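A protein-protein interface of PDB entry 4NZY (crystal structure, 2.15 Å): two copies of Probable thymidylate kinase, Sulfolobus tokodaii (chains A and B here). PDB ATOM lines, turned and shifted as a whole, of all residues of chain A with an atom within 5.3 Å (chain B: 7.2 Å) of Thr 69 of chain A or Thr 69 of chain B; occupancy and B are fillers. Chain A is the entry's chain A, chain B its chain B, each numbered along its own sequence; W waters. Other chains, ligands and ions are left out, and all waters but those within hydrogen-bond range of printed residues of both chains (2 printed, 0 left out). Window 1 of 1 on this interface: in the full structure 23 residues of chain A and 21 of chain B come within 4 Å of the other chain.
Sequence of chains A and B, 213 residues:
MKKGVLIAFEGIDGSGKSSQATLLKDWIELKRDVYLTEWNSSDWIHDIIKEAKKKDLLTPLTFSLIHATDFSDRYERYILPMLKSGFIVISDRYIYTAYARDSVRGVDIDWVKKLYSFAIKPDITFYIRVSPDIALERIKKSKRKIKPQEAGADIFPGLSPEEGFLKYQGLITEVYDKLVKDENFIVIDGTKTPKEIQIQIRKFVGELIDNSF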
ATOM      1  N   ILE A  45     -26.271 -17.093  20.833  1.00  0.00           N
ATOM      2  CA  ILE A  45     -25.734 -15.940  20.094  1.00  0.00           C
ATOM      3  C   ILE A  45     -25.303 -16.355  18.695  1.00  0.00           C
ATOM      4  O   ILE A  45     -25.646 -15.704  17.700  1.00  0.00           O
ATOM      5  CB  ILE A  45     -24.573 -15.249  20.837  1.00  0.00           C
ATOM      6  CG1 ILE A  45     -25.119 -14.552  22.088  1.00  0.00           C
ATOM      7  CG2 ILE A  45     -23.883 -14.261  19.906  1.00  0.00           C
ATOM      8  CD1 ILE A  45     -24.086 -14.072  23.091  1.00  0.00           C
ATOM      9  N   ILE A  49     -26.898 -14.462  15.169  1.00  0.00           N
ATOM     10  CA  ILE A  49     -26.081 -13.746  14.214  1.00  0.00           C
ATOM     11  C   ILE A  49     -26.078 -14.447  12.862  1.00  0.00           C
ATOM     12  O   ILE A  49     -26.283 -13.800  11.850  1.00  0.00           O
ATOM     13  CB  ILE A  49     -24.630 -13.572  14.672  1.00  0.00           C
ATOM     14  CG1 ILE A  49     -24.568 -12.873  16.030  1.00  0.00           C
ATOM     15  CG2 ILE A  49     -23.858 -12.761  13.628  1.00  0.00           C
ATOM     16  CD1 ILE A  49     -23.171 -12.724  16.583  1.00  0.00           C
ATOM     17  N   THR A  62     -15.003 -12.454  10.359  1.00  0.00           N
ATOM     18  CA  THR A  62     -16.335 -12.350  10.968  1.00  0.00           C
ATOM     19  C   THR A  62     -16.806 -13.711  11.546  1.00  0.00           C
ATOM     20  O   THR A  62     -17.325 -13.754  12.657  1.00  0.00           O
ATOM     21  CB  THR A  62     -17.337 -11.777   9.963  1.00  0.00           C
ATOM     22  OG1 THR A  62     -16.855 -10.500   9.489  1.00  0.00           O
ATOM     23  CG2 THR A  62     -18.727 -11.621  10.614  1.00  0.00           C
ATOM     24  N   SER A  64     -14.732 -15.997  12.618  1.00  0.00           N
ATOM     25  CA  SER A  64     -13.870 -16.106  13.790  1.00  0.00           C
ATOM     26  C   SER A  64     -14.492 -15.378  14.989  1.00  0.00           C
ATOM     27  O   SER A  64     -14.504 -15.900  16.100  1.00  0.00           O
ATOM     28  CB  SER A  64     -12.487 -15.547  13.506  1.00  0.00           C
ATOM     29  OG  SER A  64     -11.663 -15.677  14.642  1.00  0.00           O
ATOM     30  N   LEU A  65     -15.030 -14.185  14.744  1.00  0.00           N
ATOM     31  CA  LEU A  65     -15.577 -13.350  15.820  1.00  0.00           C
ATOM     32  C   LEU A  65     -16.941 -13.833  16.305  1.00  0.00           C
ATOM     33  O   LEU A  65     -17.234 -13.729  17.485  1.00  0.00           O
ATOM     34  CB  LEU A  65     -15.640 -11.891  15.403  1.00  0.00           C
ATOM     35  CG  LEU A  65     -14.286 -11.188  15.438  1.00  0.00           C
ATOM     36  CD1 LEU A  65     -14.278  -9.939  14.553  1.00  0.00           C
ATOM     37  CD2 LEU A  65     -13.889 -10.831  16.858  1.00  0.00           C
ATOM     38  N   ILE A  66     -17.767 -14.374  15.414  1.00  0.00           N
ATOM     39  CA  ILE A  66     -19.050 -14.944  15.828  1.00  0.00           C
ATOM     40  C   ILE A  66     -18.800 -16.074  16.833  1.00  0.00           C
ATOM     41  O   ILE A  66     -19.432 -16.140  17.875  1.00  0.00           O
ATOM     42  CB  ILE A  66     -19.863 -15.489  14.646  1.00  0.00           C
ATOM     43  CG1 ILE A  66     -20.400 -14.329  13.810  1.00  0.00           C
ATOM     44  CG2 ILE A  66     -21.029 -16.348  15.150  1.00  0.00           C
ATOM     45  CD1 ILE A  66     -20.975 -14.728  12.467  1.00  0.00           C
ATOM     46  N   HIS A  67     -17.839 -16.928  16.527  1.00  0.00           N
ATOM     47  CA  HIS A  67     -17.549 -18.070  17.371  1.00  0.00           C
ATOM     48  C   HIS A  67     -16.913 -17.678  18.697  1.00  0.00           C
ATOM     49  O   HIS A  67     -17.234 -18.257  19.723  1.00  0.00           O
ATOM     50  CB  HIS A  67     -16.681 -19.067  16.620  1.00  0.00           C
ATOM     51  CG  HIS A  67     -17.294 -19.541  15.345  1.00  0.00           C
ATOM     52  ND1 HIS A  67     -16.564 -20.167  14.353  1.00  0.00           N
ATOM     53  CD2 HIS A  67     -18.570 -19.478  14.894  1.00  0.00           C
ATOM     54  CE1 HIS A  67     -17.366 -20.473  13.347  1.00  0.00           C
ATOM     55  NE2 HIS A  67     -18.588 -20.066  13.652  1.00  0.00           N
ATOM     56  N   ALA A  68     -16.026 -16.689  18.687  1.00  0.00           N
ATOM     57  CA  ALA A  68     -15.435 -16.242  19.930  1.00  0.00           C
ATOM     58  C   ALA A  68     -16.506 -15.597  20.803  1.00  0.00           C
ATOM     59  O   ALA A  68     -16.522 -15.800  22.019  1.00  0.00           O
ATOM     60  CB  ALA A  68     -14.265 -15.288  19.686  1.00  0.00           C
ATOM     61  N   THR A  69     -17.415 -14.857  20.172  1.00  0.00           N
ATOM     62  CA  THR A  69     -18.515 -14.212  20.888  1.00  0.00           C
ATOM     63  C   THR A  69     -19.419 -15.234  21.551  1.00  0.00           C
ATOM     64  O   THR A  69     -19.725 -15.130  22.739  1.00  0.00           O
ATOM     65  CB  THR A  69     -19.381 -13.340  19.956  1.00  0.00           C
ATOM     66  OG1 THR A  69     -18.552 -12.393  19.283  1.00  0.00           O
ATOM     67  CG2 THR A  69     -20.424 -12.575  20.756  1.00  0.00           C
ATOM     68  N   ASP A  70     -19.854 -16.220  20.771  1.00  0.00           N
ATOM     69  CA  ASP A  70     -20.721 -17.259  21.289  1.00  0.00           C
ATOM     70  C   ASP A  70     -19.971 -17.995  22.395  1.00  0.00           C
ATOM     71  O   ASP A  70     -20.511 -18.208  23.483  1.00  0.00           O
ATOM     72  CB  ASP A  70     -21.137 -18.205  20.161  1.00  0.00           C
ATOM     73  CG  ASP A  70     -22.164 -19.223  20.598  1.00  0.00           C
ATOM     74  OD1 ASP A  70     -23.360 -18.865  20.803  1.00  0.00           O
ATOM     75  OD2 ASP A  70     -21.774 -20.405  20.707  1.00  0.00           O
ATOM     76  N   PHE A  71     -18.710 -18.349  22.146  1.00  0.00           N
ATOM     77  CA  PHE A  71     -17.933 -19.009  23.188  1.00  0.00           C
ATOM     78  C   PHE A  71     -17.752 -18.181  24.470  1.00  0.00           C
ATOM     79  O   PHE A  71     -17.739 -18.764  25.559  1.00  0.00           O
ATOM     80  CB  PHE A  71     -16.565 -19.481  22.720  1.00  0.00           C
ATOM     81  CG  PHE A  71     -15.853 -20.295  23.757  1.00  0.00           C
ATOM     82  CD1 PHE A  71     -16.405 -21.493  24.198  1.00  0.00           C
ATOM     83  CD2 PHE A  71     -14.684 -19.846  24.339  1.00  0.00           C
ATOM     84  CE1 PHE A  71     -15.784 -22.242  25.189  1.00  0.00           C
ATOM     85  CE2 PHE A  71     -14.051 -20.589  25.322  1.00  0.00           C
ATOM     86  CZ  PHE A  71     -14.595 -21.788  25.742  1.00  0.00           C
ATOM     87  N   SER A  72     -17.579 -16.858  24.360  1.00  0.00           N
ATOM     88  CA  SER A  72     -17.430 -16.026  25.566  1.00  0.00           C
ATOM     89  C   SER A  72     -18.653 -16.172  26.460  1.00  0.00           C
ATOM     90  O   SER A  72     -18.521 -16.197  27.674  1.00  0.00           O
ATOM     91  CB  SER A  72     -17.205 -14.550  25.252  1.00  0.00           C
ATOM     92  OG  SER A  72     -18.363 -13.938  24.707  1.00  0.00           O
ATOM     93  N   ASP A  73     -19.834 -16.288  25.862  1.00  0.00           N
ATOM     94  CA  ASP A  73     -21.056 -16.461  26.652  1.00  0.00           C
ATOM     95  C   ASP A  73     -21.120 -17.869  27.272  1.00  0.00           C
ATOM     96  O   ASP A  73     -21.414 -18.015  28.455  1.00  0.00           O
ATOM     97  CB  ASP A  73     -22.284 -16.163  25.806  1.00  0.00           C
ATOM     98  CG  ASP A  73     -23.576 -16.176  26.617  1.00  0.00           C
ATOM     99  OD1 ASP A  73     -23.845 -15.167  27.308  1.00  0.00           O
ATOM    100  OD2 ASP A  73     -24.348 -17.164  26.534  1.00  0.00           O
ATOM    101  N   TRP B  44     -29.790  -7.456  14.500  1.00  0.00           N
ATOM    102  CA  TRP B  44     -29.452  -8.610  15.331  1.00  0.00           C
ATOM    103  C   TRP B  44     -28.808  -8.256  16.669  1.00  0.00           C
ATOM    104  O   TRP B  44     -29.014  -8.962  17.642  1.00  0.00           O
ATOM    105  CB  TRP B  44     -28.585  -9.608  14.567  1.00  0.00           C
ATOM    106  CG  TRP B  44     -27.302  -9.098  13.966  1.00  0.00           C
ATOM    107  CD1 TRP B  44     -27.108  -8.673  12.674  1.00  0.00           C
ATOM    108  CD2 TRP B  44     -26.017  -9.037  14.600  1.00  0.00           C
ATOM    109  NE1 TRP B  44     -25.791  -8.343  12.475  1.00  0.00           N
ATOM    110  CE2 TRP B  44     -25.098  -8.557  13.638  1.00  0.00           C
ATOM    111  CE3 TRP B  44     -25.556  -9.333  15.879  1.00  0.00           C
ATOM    112  CZ2 TRP B  44     -23.740  -8.360  13.928  1.00  0.00           C
ATOM    113  CZ3 TRP B  44     -24.204  -9.146  16.164  1.00  0.00           C
ATOM    114  CH2 TRP B  44     -23.314  -8.664  15.190  1.00  0.00           C
ATOM    115  N   ILE B  45     -28.049  -7.164  16.733  1.00  0.00           N
ATOM    116  CA  ILE B  45     -27.480  -6.740  18.018  1.00  0.00           C
ATOM    117  C   ILE B  45     -28.609  -6.481  19.019  1.00  0.00           C
ATOM    118  O   ILE B  45     -28.567  -6.966  20.148  1.00  0.00           O
ATOM    119  CB  ILE B  45     -26.589  -5.488  17.891  1.00  0.00           C
ATOM    120  CG1 ILE B  45     -25.317  -5.834  17.118  1.00  0.00           C
ATOM    121  CG2 ILE B  45     -26.248  -4.931  19.275  1.00  0.00           C
ATOM    122  CD1 ILE B  45     -24.399  -4.651  16.882  1.00  0.00           C
ATOM    123  N   ILE B  48     -29.989  -9.743  20.121  1.00  0.00           N
ATOM    124  CA  ILE B  48     -29.131 -10.406  21.096  1.00  0.00           C
ATOM    125  C   ILE B  48     -29.352  -9.847  22.499  1.00  0.00           C
ATOM    126  O   ILE B  48     -29.423 -10.616  23.468  1.00  0.00           O
ATOM    127  CB  ILE B  48     -27.630 -10.325  20.729  1.00  0.00           C
ATOM    128  CG1 ILE B  48     -27.330 -11.253  19.549  1.00  0.00           C
ATOM    129  CG2 ILE B  48     -26.752 -10.705  21.926  1.00  0.00           C
ATOM    130  CD1 ILE B  48     -25.949 -11.063  18.959  1.00  0.00           C
ATOM    131  N   LEU B  58     -25.371 -10.967  30.201  1.00  0.00           N
ATOM    132  CA  LEU B  58     -24.556 -10.542  29.070  1.00  0.00           C
ATOM    133  C   LEU B  58     -23.358  -9.823  29.681  1.00  0.00           C
ATOM    134  O   LEU B  58     -23.513  -8.721  30.219  1.00  0.00           O
ATOM    135  CB  LEU B  58     -25.325  -9.615  28.124  1.00  0.00           C
ATOM    136  CG  LEU B  58     -24.630  -9.318  26.787  1.00  0.00           C
ATOM    137  CD1 LEU B  58     -24.627 -10.543  25.891  1.00  0.00           C
ATOM    138  CD2 LEU B  58     -25.274  -8.141  26.057  1.00  0.00           C
ATOM    139  N   LEU B  61     -17.444  -8.523  28.321  1.00  0.00           N
ATOM    140  CA  LEU B  61     -16.666  -9.266  27.322  1.00  0.00           C
ATOM    141  C   LEU B  61     -17.490  -9.613  26.084  1.00  0.00           C
ATOM    142  O   LEU B  61     -17.122  -9.279  24.962  1.00  0.00           O
ATOM    143  CB  LEU B  61     -16.094 -10.540  27.953  1.00  0.00           C
ATOM    144  CG  LEU B  61     -15.437 -11.551  26.994  1.00  0.00           C
ATOM    145  CD1 LEU B  61     -14.387 -10.863  26.136  1.00  0.00           C
ATOM    146  CD2 LEU B  61     -14.811 -12.707  27.761  1.00  0.00           C
ATOM    147  N   THR B  62     -18.624 -10.260  26.304  1.00  0.00           N
ATOM    148  CA  THR B  62     -19.488 -10.675  25.224  1.00  0.00           C
ATOM    149  C   THR B  62     -20.064  -9.461  24.491  1.00  0.00           C
ATOM    150  O   THR B  62     -20.167  -9.464  23.276  1.00  0.00           O
ATOM    151  CB  THR B  62     -20.608 -11.598  25.757  1.00  0.00           C
ATOM    152  OG1 THR B  62     -20.033 -12.779  26.363  1.00  0.00           O
ATOM    153  CG2 THR B  62     -21.535 -12.004  24.648  1.00  0.00           C
ATOM    154  N   PHE B  63     -20.410  -8.413  25.232  1.00  0.00           N
ATOM    155  CA  PHE B  63     -20.910  -7.155  24.642  1.00  0.00           C
ATOM    156  C   PHE B  63     -19.881  -6.553  23.690  1.00  0.00           C
ATOM    157  O   PHE B  63     -20.210  -6.151  22.574  1.00  0.00           O
ATOM    158  CB  PHE B  63     -21.222  -6.153  25.771  1.00  0.00           C
ATOM    159  CG  PHE B  63     -21.955  -4.908  25.323  1.00  0.00           C
ATOM    160  CD1 PHE B  63     -21.511  -3.641  25.726  1.00  0.00           C
ATOM    161  CD2 PHE B  63     -23.099  -4.992  24.538  1.00  0.00           C
ATOM    162  CE1 PHE B  63     -22.194  -2.490  25.353  1.00  0.00           C
ATOM    163  CE2 PHE B  63     -23.788  -3.836  24.152  1.00  0.00           C
ATOM    164  CZ  PHE B  63     -23.330  -2.579  24.564  1.00  0.00           C
ATOM    165  N   SER B  64     -18.634  -6.504  24.146  1.00  0.00           N
ATOM    166  CA  SER B  64     -17.489  -6.062  23.329  1.00  0.00           C
ATOM    167  C   SER B  64     -17.367  -6.884  22.042  1.00  0.00           C
ATOM    168  O   SER B  64     -17.171  -6.337  20.945  1.00  0.00           O
ATOM    169  CB  SER B  64     -16.195  -6.155  24.161  1.00  0.00           C
ATOM    170  OG  SER B  64     -15.014  -5.936  23.402  1.00  0.00           O
ATOM    171  N   LEU B  65     -17.502  -8.196  22.168  1.00  0.00           N
ATOM    172  CA  LEU B  65     -17.282  -9.098  21.040  1.00  0.00           C
ATOM    173  C   LEU B  65     -18.447  -9.041  20.042  1.00  0.00           C
ATOM    174  O   LEU B  65     -18.243  -9.113  18.831  1.00  0.00           O
ATOM    175  CB  LEU B  65     -17.022 -10.521  21.552  1.00  0.00           C
ATOM    176  CG  LEU B  65     -15.623 -10.771  22.130  1.00  0.00           C
ATOM    177  CD1 LEU B  65     -15.562 -12.104  22.868  1.00  0.00           C
ATOM    178  CD2 LEU B  65     -14.549 -10.725  21.039  1.00  0.00           C
ATOM    179  N   ILE B  66     -19.662  -8.849  20.543  1.00  0.00           N
ATOM    180  CA  ILE B  66     -20.819  -8.654  19.666  1.00  0.00           C
ATOM    181  C   ILE B  66     -20.620  -7.462  18.740  1.00  0.00           C
ATOM    182  O   ILE B  66     -20.860  -7.543  17.541  1.00  0.00           O
ATOM    183  CB  ILE B  66     -22.104  -8.424  20.489  1.00  0.00           C
ATOM    184  CG1 ILE B  66     -22.580  -9.742  21.079  1.00  0.00           C
ATOM    185  CG2 ILE B  66     -23.182  -7.783  19.641  1.00  0.00           C
ATOM    186  CD1 ILE B  66     -23.473  -9.546  22.302  1.00  0.00           C
ATOM    187  N   HIS B  67     -20.186  -6.350  19.310  1.00  0.00           N
ATOM    188  CA  HIS B  67     -19.928  -5.144  18.531  1.00  0.00           C
ATOM    189  C   HIS B  67     -18.743  -5.270  17.596  1.00  0.00           C
ATOM    190  O   HIS B  67     -18.796  -4.760  16.489  1.00  0.00           O
ATOM    191  CB  HIS B  67     -19.734  -3.958  19.464  1.00  0.00           C
ATOM    192  CG  HIS B  67     -21.024  -3.376  19.912  1.00  0.00           C
ATOM    193  ND1 HIS B  67     -21.542  -3.584  21.171  1.00  0.00           N
ATOM    194  CD2 HIS B  67     -21.932  -2.627  19.247  1.00  0.00           C
ATOM    195  CE1 HIS B  67     -22.705  -2.969  21.267  1.00  0.00           C
ATOM    196  NE2 HIS B  67     -22.966  -2.386  20.114  1.00  0.00           N
ATOM    197  N   ALA B  68     -17.698  -5.982  18.005  1.00  0.00           N
ATOM    198  CA  ALA B  68     -16.533  -6.176  17.123  1.00  0.00           C
ATOM    199  C   ALA B  68     -16.936  -7.011  15.918  1.00  0.00           C
ATOM    200  O   ALA B  68     -16.553  -6.708  14.798  1.00  0.00           O
ATOM    201  CB  ALA B  68     -15.374  -6.832  17.867  1.00  0.00           C
ATOM    202  N   THR B  69     -17.744  -8.042  16.163  1.00  0.00           N
ATOM    203  CA  THR B  69     -18.270  -8.891  15.099  1.00  0.00           C
ATOM    204  C   THR B  69     -19.025  -8.062  14.058  1.00  0.00           C
ATOM    205  O   THR B  69     -18.798  -8.207  12.867  1.00  0.00           O
ATOM    206  CB  THR B  69     -19.216  -9.955  15.659  1.00  0.00           C
ATOM    207  OG1 THR B  69     -18.537 -10.745  16.658  1.00  0.00           O
ATOM    208  CG2 THR B  69     -19.746 -10.842  14.526  1.00  0.00           C
ATOM    209  N   ASP B  70     -19.929  -7.204  14.524  1.00  0.00           N
ATOM    210  CA  ASP B  70     -20.710  -6.336  13.639  1.00  0.00           C
ATOM    211  C   ASP B  70     -19.802  -5.402  12.850  1.00  0.00           C
ATOM    212  O   ASP B  70     -19.919  -5.291  11.635  1.00  0.00           O
ATOM    213  CB  ASP B  70     -21.691  -5.511  14.458  1.00  0.00           C
ATOM    214  CG  ASP B  70     -22.669  -4.721  13.596  1.00  0.00           C
ATOM    215  OD1 ASP B  70     -23.080  -5.208  12.531  1.00  0.00           O
ATOM    216  OD2 ASP B  70     -23.038  -3.610  13.999  1.00  0.00           O
ATOM    217  N   PHE B  71     -18.891  -4.747  13.561  1.00  0.00           N
ATOM    218  CA  PHE B  71     -17.928  -3.865  12.946  1.00  0.00           C
ATOM    219  C   PHE B  71     -17.040  -4.575  11.931  1.00  0.00           C
ATOM    220  O   PHE B  71     -16.765  -4.005  10.880  1.00  0.00           O
ATOM    221  CB  PHE B  71     -17.046  -3.186  14.005  1.00  0.00           C
ATOM    222  CG  PHE B  71     -15.986  -2.305  13.418  1.00  0.00           C
ATOM    223  CD1 PHE B  71     -16.273  -0.996  13.061  1.00  0.00           C
ATOM    224  CD2 PHE B  71     -14.719  -2.795  13.176  1.00  0.00           C
ATOM    225  CE1 PHE B  71     -15.302  -0.189  12.507  1.00  0.00           C
ATOM    226  CE2 PHE B  71     -13.745  -1.997  12.618  1.00  0.00           C
ATOM    227  CZ  PHE B  71     -14.036  -0.686  12.285  1.00  0.00           C
ATOM    228  N   SER B  72     -16.594  -5.799  12.231  1.00  0.00           N
ATOM    229  CA  SER B  72     -15.757  -6.549  11.266  1.00  0.00           C
ATOM    230  C   SER B  72     -16.481  -6.755   9.951  1.00  0.00           C
ATOM    231  O   SER B  72     -15.877  -6.703   8.888  1.00  0.00           O
ATOM    232  CB  SER B  72     -15.323  -7.918  11.816  1.00  0.00           C
ATOM    233  OG  SER B  72     -16.419  -8.815  11.932  1.00  0.00           O
ATOM    234  N   ASP B  73     -17.784  -6.994  10.034  1.00  0.00           N
ATOM    235  CA  ASP B  73     -18.589  -7.246   8.854  1.00  0.00           C
ATOM    236  C   ASP B  73     -18.757  -5.958   8.015  1.00  0.00           C
ATOM    237  O   ASP B  73     -18.546  -5.972   6.812  1.00  0.00           O
ATOM    238  CB  ASP B  73     -19.936  -7.820   9.270  1.00  0.00           C
ATOM    239  CG  ASP B  73     -20.799  -8.191   8.084  1.00  0.00           C
ATOM    240  OD1 ASP B  73     -20.373  -9.012   7.242  1.00  0.00           O
ATOM    241  OD2 ASP B  73     -21.918  -7.665   8.013  1.00  0.00           O
ATOM    242  N   ARG B  74     -19.104  -4.857   8.667  1.00  0.00           N
ATOM    243  CA  ARG B  74     -19.213  -3.555   7.994  1.00  0.00           C
ATOM    244  C   ARG B  74     -17.855  -3.112   7.454  1.00  0.00           C
ATOM    245  O   ARG B  74     -17.774  -2.552   6.363  1.00  0.00           O
ATOM    246  CB  ARG B  74     -19.785  -2.481   8.945  1.00  0.00           C
ATOM    247  CG  ARG B  74     -21.014  -2.938   9.734  1.00  0.00           C
ATOM    248  CD  ARG B  74     -21.909  -1.798  10.223  1.00  0.00           C
ATOM    249  NE  ARG B  74     -23.174  -2.316  10.745  1.00  0.00           N
ATOM    250  CZ  ARG B  74     -24.214  -1.562  11.094  1.00  0.00           C
ATOM    251  N   TYR B  75     -16.790  -3.391   8.209  1.00  0.00           N
ATOM    252  CA  TYR B  75     -15.437  -3.058   7.784  1.00  0.00           C
ATOM    253  C   TYR B  75     -15.025  -3.852   6.542  1.00  0.00           C
ATOM    254  O   TYR B  75     -14.587  -3.277   5.541  1.00  0.00           O
ATOM    255  CB  TYR B  75     -14.416  -3.293   8.913  1.00  0.00           C
ATOM    256  CG  TYR B  75     -13.013  -2.836   8.558  1.00  0.00           C
ATOM    257  CD1 TYR B  75     -12.670  -1.475   8.572  1.00  0.00           C
ATOM    258  CD2 TYR B  75     -12.033  -3.756   8.193  1.00  0.00           C
ATOM    259  CE1 TYR B  75     -11.394  -1.066   8.239  1.00  0.00           C
ATOM    260  CE2 TYR B  75     -10.747  -3.353   7.871  1.00  0.00           C
ATOM    261  CZ  TYR B  75     -10.439  -2.014   7.876  1.00  0.00           C
ATOM    262  OH  TYR B  75      -9.148  -1.629   7.550  1.00  0.00           O
ATOM    263  N   LEU B 115      -7.972  -6.480  19.617  1.00  0.00           N
ATOM    264  CA  LEU B 115      -9.192  -6.979  18.984  1.00  0.00           C
ATOM    265  C   LEU B 115      -9.496  -6.248  17.666  1.00  0.00           C
ATOM    266  O   LEU B 115      -9.735  -6.888  16.630  1.00  0.00           O
ATOM    267  CB  LEU B 115     -10.375  -6.842  19.951  1.00  0.00           C
ATOM    268  CG  LEU B 115     -11.745  -7.289  19.443  1.00  0.00           C
ATOM    269  CD1 LEU B 115     -11.761  -8.787  19.153  1.00  0.00           C
ATOM    270  CD2 LEU B 115     -12.820  -6.909  20.451  1.00  0.00           C
ATOM    271  N   TYR B 116      -9.480  -4.909  17.710  1.00  0.00           N
ATOM    272  CA  TYR B 116      -9.799  -4.110  16.524  1.00  0.00           C
ATOM    273  C   TYR B 116      -8.592  -3.839  15.613  1.00  0.00           C
ATOM    274  O   TYR B 116      -8.703  -3.037  14.686  1.00  0.00           O
ATOM    275  CB  TYR B 116     -10.450  -2.768  16.940  1.00  0.00           C
ATOM    276  CG  TYR B 116     -11.894  -2.898  17.348  1.00  0.00           C
ATOM    277  CD1 TYR B 116     -12.907  -2.866  16.404  1.00  0.00           C
ATOM    278  CD2 TYR B 116     -12.249  -3.083  18.679  1.00  0.00           C
ATOM    279  CE1 TYR B 116     -14.248  -2.993  16.779  1.00  0.00           C
ATOM    280  CE2 TYR B 116     -13.583  -3.218  19.063  1.00  0.00           C
ATOM    281  CZ  TYR B 116     -14.577  -3.174  18.113  1.00  0.00           C
ATOM    282  OH  TYR B 116     -15.894  -3.312  18.509  1.00  0.00           O
ATOM    283  N   PHE B 118      -7.285  -5.346  13.248  1.00  0.00           N
ATOM    284  CA  PHE B 118      -7.493  -5.623  11.837  1.00  0.00           C
ATOM    285  C   PHE B 118      -7.868  -4.382  11.019  1.00  0.00           C
ATOM    286  O   PHE B 118      -7.788  -4.402   9.793  1.00  0.00           O
ATOM    287  CB  PHE B 118      -8.547  -6.713  11.642  1.00  0.00           C
ATOM    288  CG  PHE B 118      -9.897  -6.391  12.224  1.00  0.00           C
ATOM    289  CD1 PHE B 118     -10.804  -5.614  11.524  1.00  0.00           C
ATOM    290  CD2 PHE B 118     -10.287  -6.933  13.444  1.00  0.00           C
ATOM    291  CE1 PHE B 118     -12.057  -5.356  12.037  1.00  0.00           C
ATOM    292  CE2 PHE B 118     -11.540  -6.673  13.967  1.00  0.00           C
ATOM    293  CZ  PHE B 118     -12.419  -5.873  13.269  1.00  0.00           C
HETATM  294  O   HOH W   1     -18.018 -10.627   6.993  1.00  0.00           O
HETATM  295  O   HOH W   2     -22.283 -13.114  28.145  1.00  0.00           O
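The backbone carbonyl oxygen (O) of Thr 69 of chain B is in hydrogen-bond range of the side-chain hydroxyl (OG) of Ser 72 of chain B (2.6 Å).
The backbone NH (N) of Ile 45 of chain A lies within hydrogen-bond range of the side-chain carboxylate (OD1) of Asp 70 of chain A (3.4 Å).
The backbone carbonyl oxygen (O) of Leu 65 of chain A is in hydrogen-bond range of the side-chain hydroxyl (OG1) of Thr 69 of chain A.
The backbone NH of Ala 68 of chain B lies close to the side-chain hydroxyl of Tyr 116 of chain B.
O of Leu 65 of chain B is in hydrogen-bond range of OG1 of Thr 69 of chain B, at 2.7 Å.
Water W2 bridges the side-chain carboxylate of Asp 73 of chain A and the side-chain hydroxyl of Thr 62 of chain B.
Water W1 lies within hydrogen-bond range of OG1 of Thr 62 of chain A and OD1 of Asp 73 of chain B.
Hydrophobic or aromatic side chains of chain B that line the printed part of chain A: Trp 44, Ile 48, Leu 61, Leu 65, Ile 66 and Leu 115.
Of the 13 printed residues of chain A, 9 touch a printed residue of chain B.
Hydrophobic or aromatic side chains of chain A that line the printed part of chain B: Ile 45, Ile 49, Leu 65 and Ile 66.
Among the printed residues, 19 pairs touch across the chains.
Among the printed residues, no Asp or Glu carboxylate lies within 4 Å of a Lys or Arg side-chain nitrogen of the other chain.
OG1 of Thr 69 of chain A sits close to O of Leu 65 of chain B.
OG1 of Thr 62 of chain B is in hydrogen-bond range of OG of Ser 72 of chain A, at 2.6 Å.
OG1 of Thr 69 of chain A sits at hydrogen-bond distance from OG1 of Thr 69 of chain B, at 3.1 Å.
The side-chain hydroxyl (OG1) of Thr 62 of chain A is in hydrogen-bond range of the side-chain hydroxyl (OG) of Ser 72 of chain B (3.0 Å).
The backbone carbonyl oxygen (O) of Leu 65 of chain A lies close to the side-chain hydroxyl (OG1) of Thr 69 of chain B (3.4 Å).
Thr 62 of chain A touches Ser 72 of chain B, and with the chains exchanged Ser 72 of chain A touches Thr 62 of chain B.
Leu 65 of chain A touches Thr 69 of chain B, and with the chains exchanged Thr 69 of chain A touches Leu 65 of chain B.
Leu 65 of chain A touches Ser 72 of chain B, and with the chains exchanged Ser 72 of chain A touches Leu 65 of chain B.
Ile 66 of chain A touches Thr 69 of chain B, and with the chains exchanged Thr 69 of chain A touches Ile 66 of chain B.
Of the 19 pairs that touch across the chains among the printed residues, 13 have their exchanged pair printed and touching as well.
Among the printed residues, merely in contact across the chains: Asp 73 of chain A with Thr 62 of chain B, Leu 65 of chain A with Ser 72 of chain B, Thr 69 of chain A with Ile 66 of chain B, Ile 66 of chain A with Thr 69 of chain B, Ile 45 of chain A with Thr 62 of chain B, Thr 62 of chain A with Asp 73 of chain B, Ile 49 of chain A with Trp 44 of chain B, Ile 49 of chain A with Ile 48 of chain B, Leu 65 of chain A with Leu 115 of chain B, Ser 72 of chain A with Leu 65 of chain B, Ser 72 of chain A with Leu 61 of chain B, Ala 68 of chain A with Leu 65 of chain B, Ile 45 of chain A with Ile 48 of chain B and Leu 65 of chain A with Ala 68 of chain B.
Printed residues of chain B within 4 Å of Thr 69 of chain A: Leu 65, Ile 66 and Thr 69.
Ile 45 of chain B touches none of the printed residues of chain A.
Of the printed residues of chain A, Leu 65 of chain B touches Ala 68, Thr 69 and Ser 72.
Of the printed residues of chain A, Ile 66 of chain B touches Thr 69 (3.6 Å).
Thr 69 of chain B touches just these residues of chain A: Leu 65, Ile 66 and Thr 69.
Tyr 75 of chain B touches none of the printed residues of chain A.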
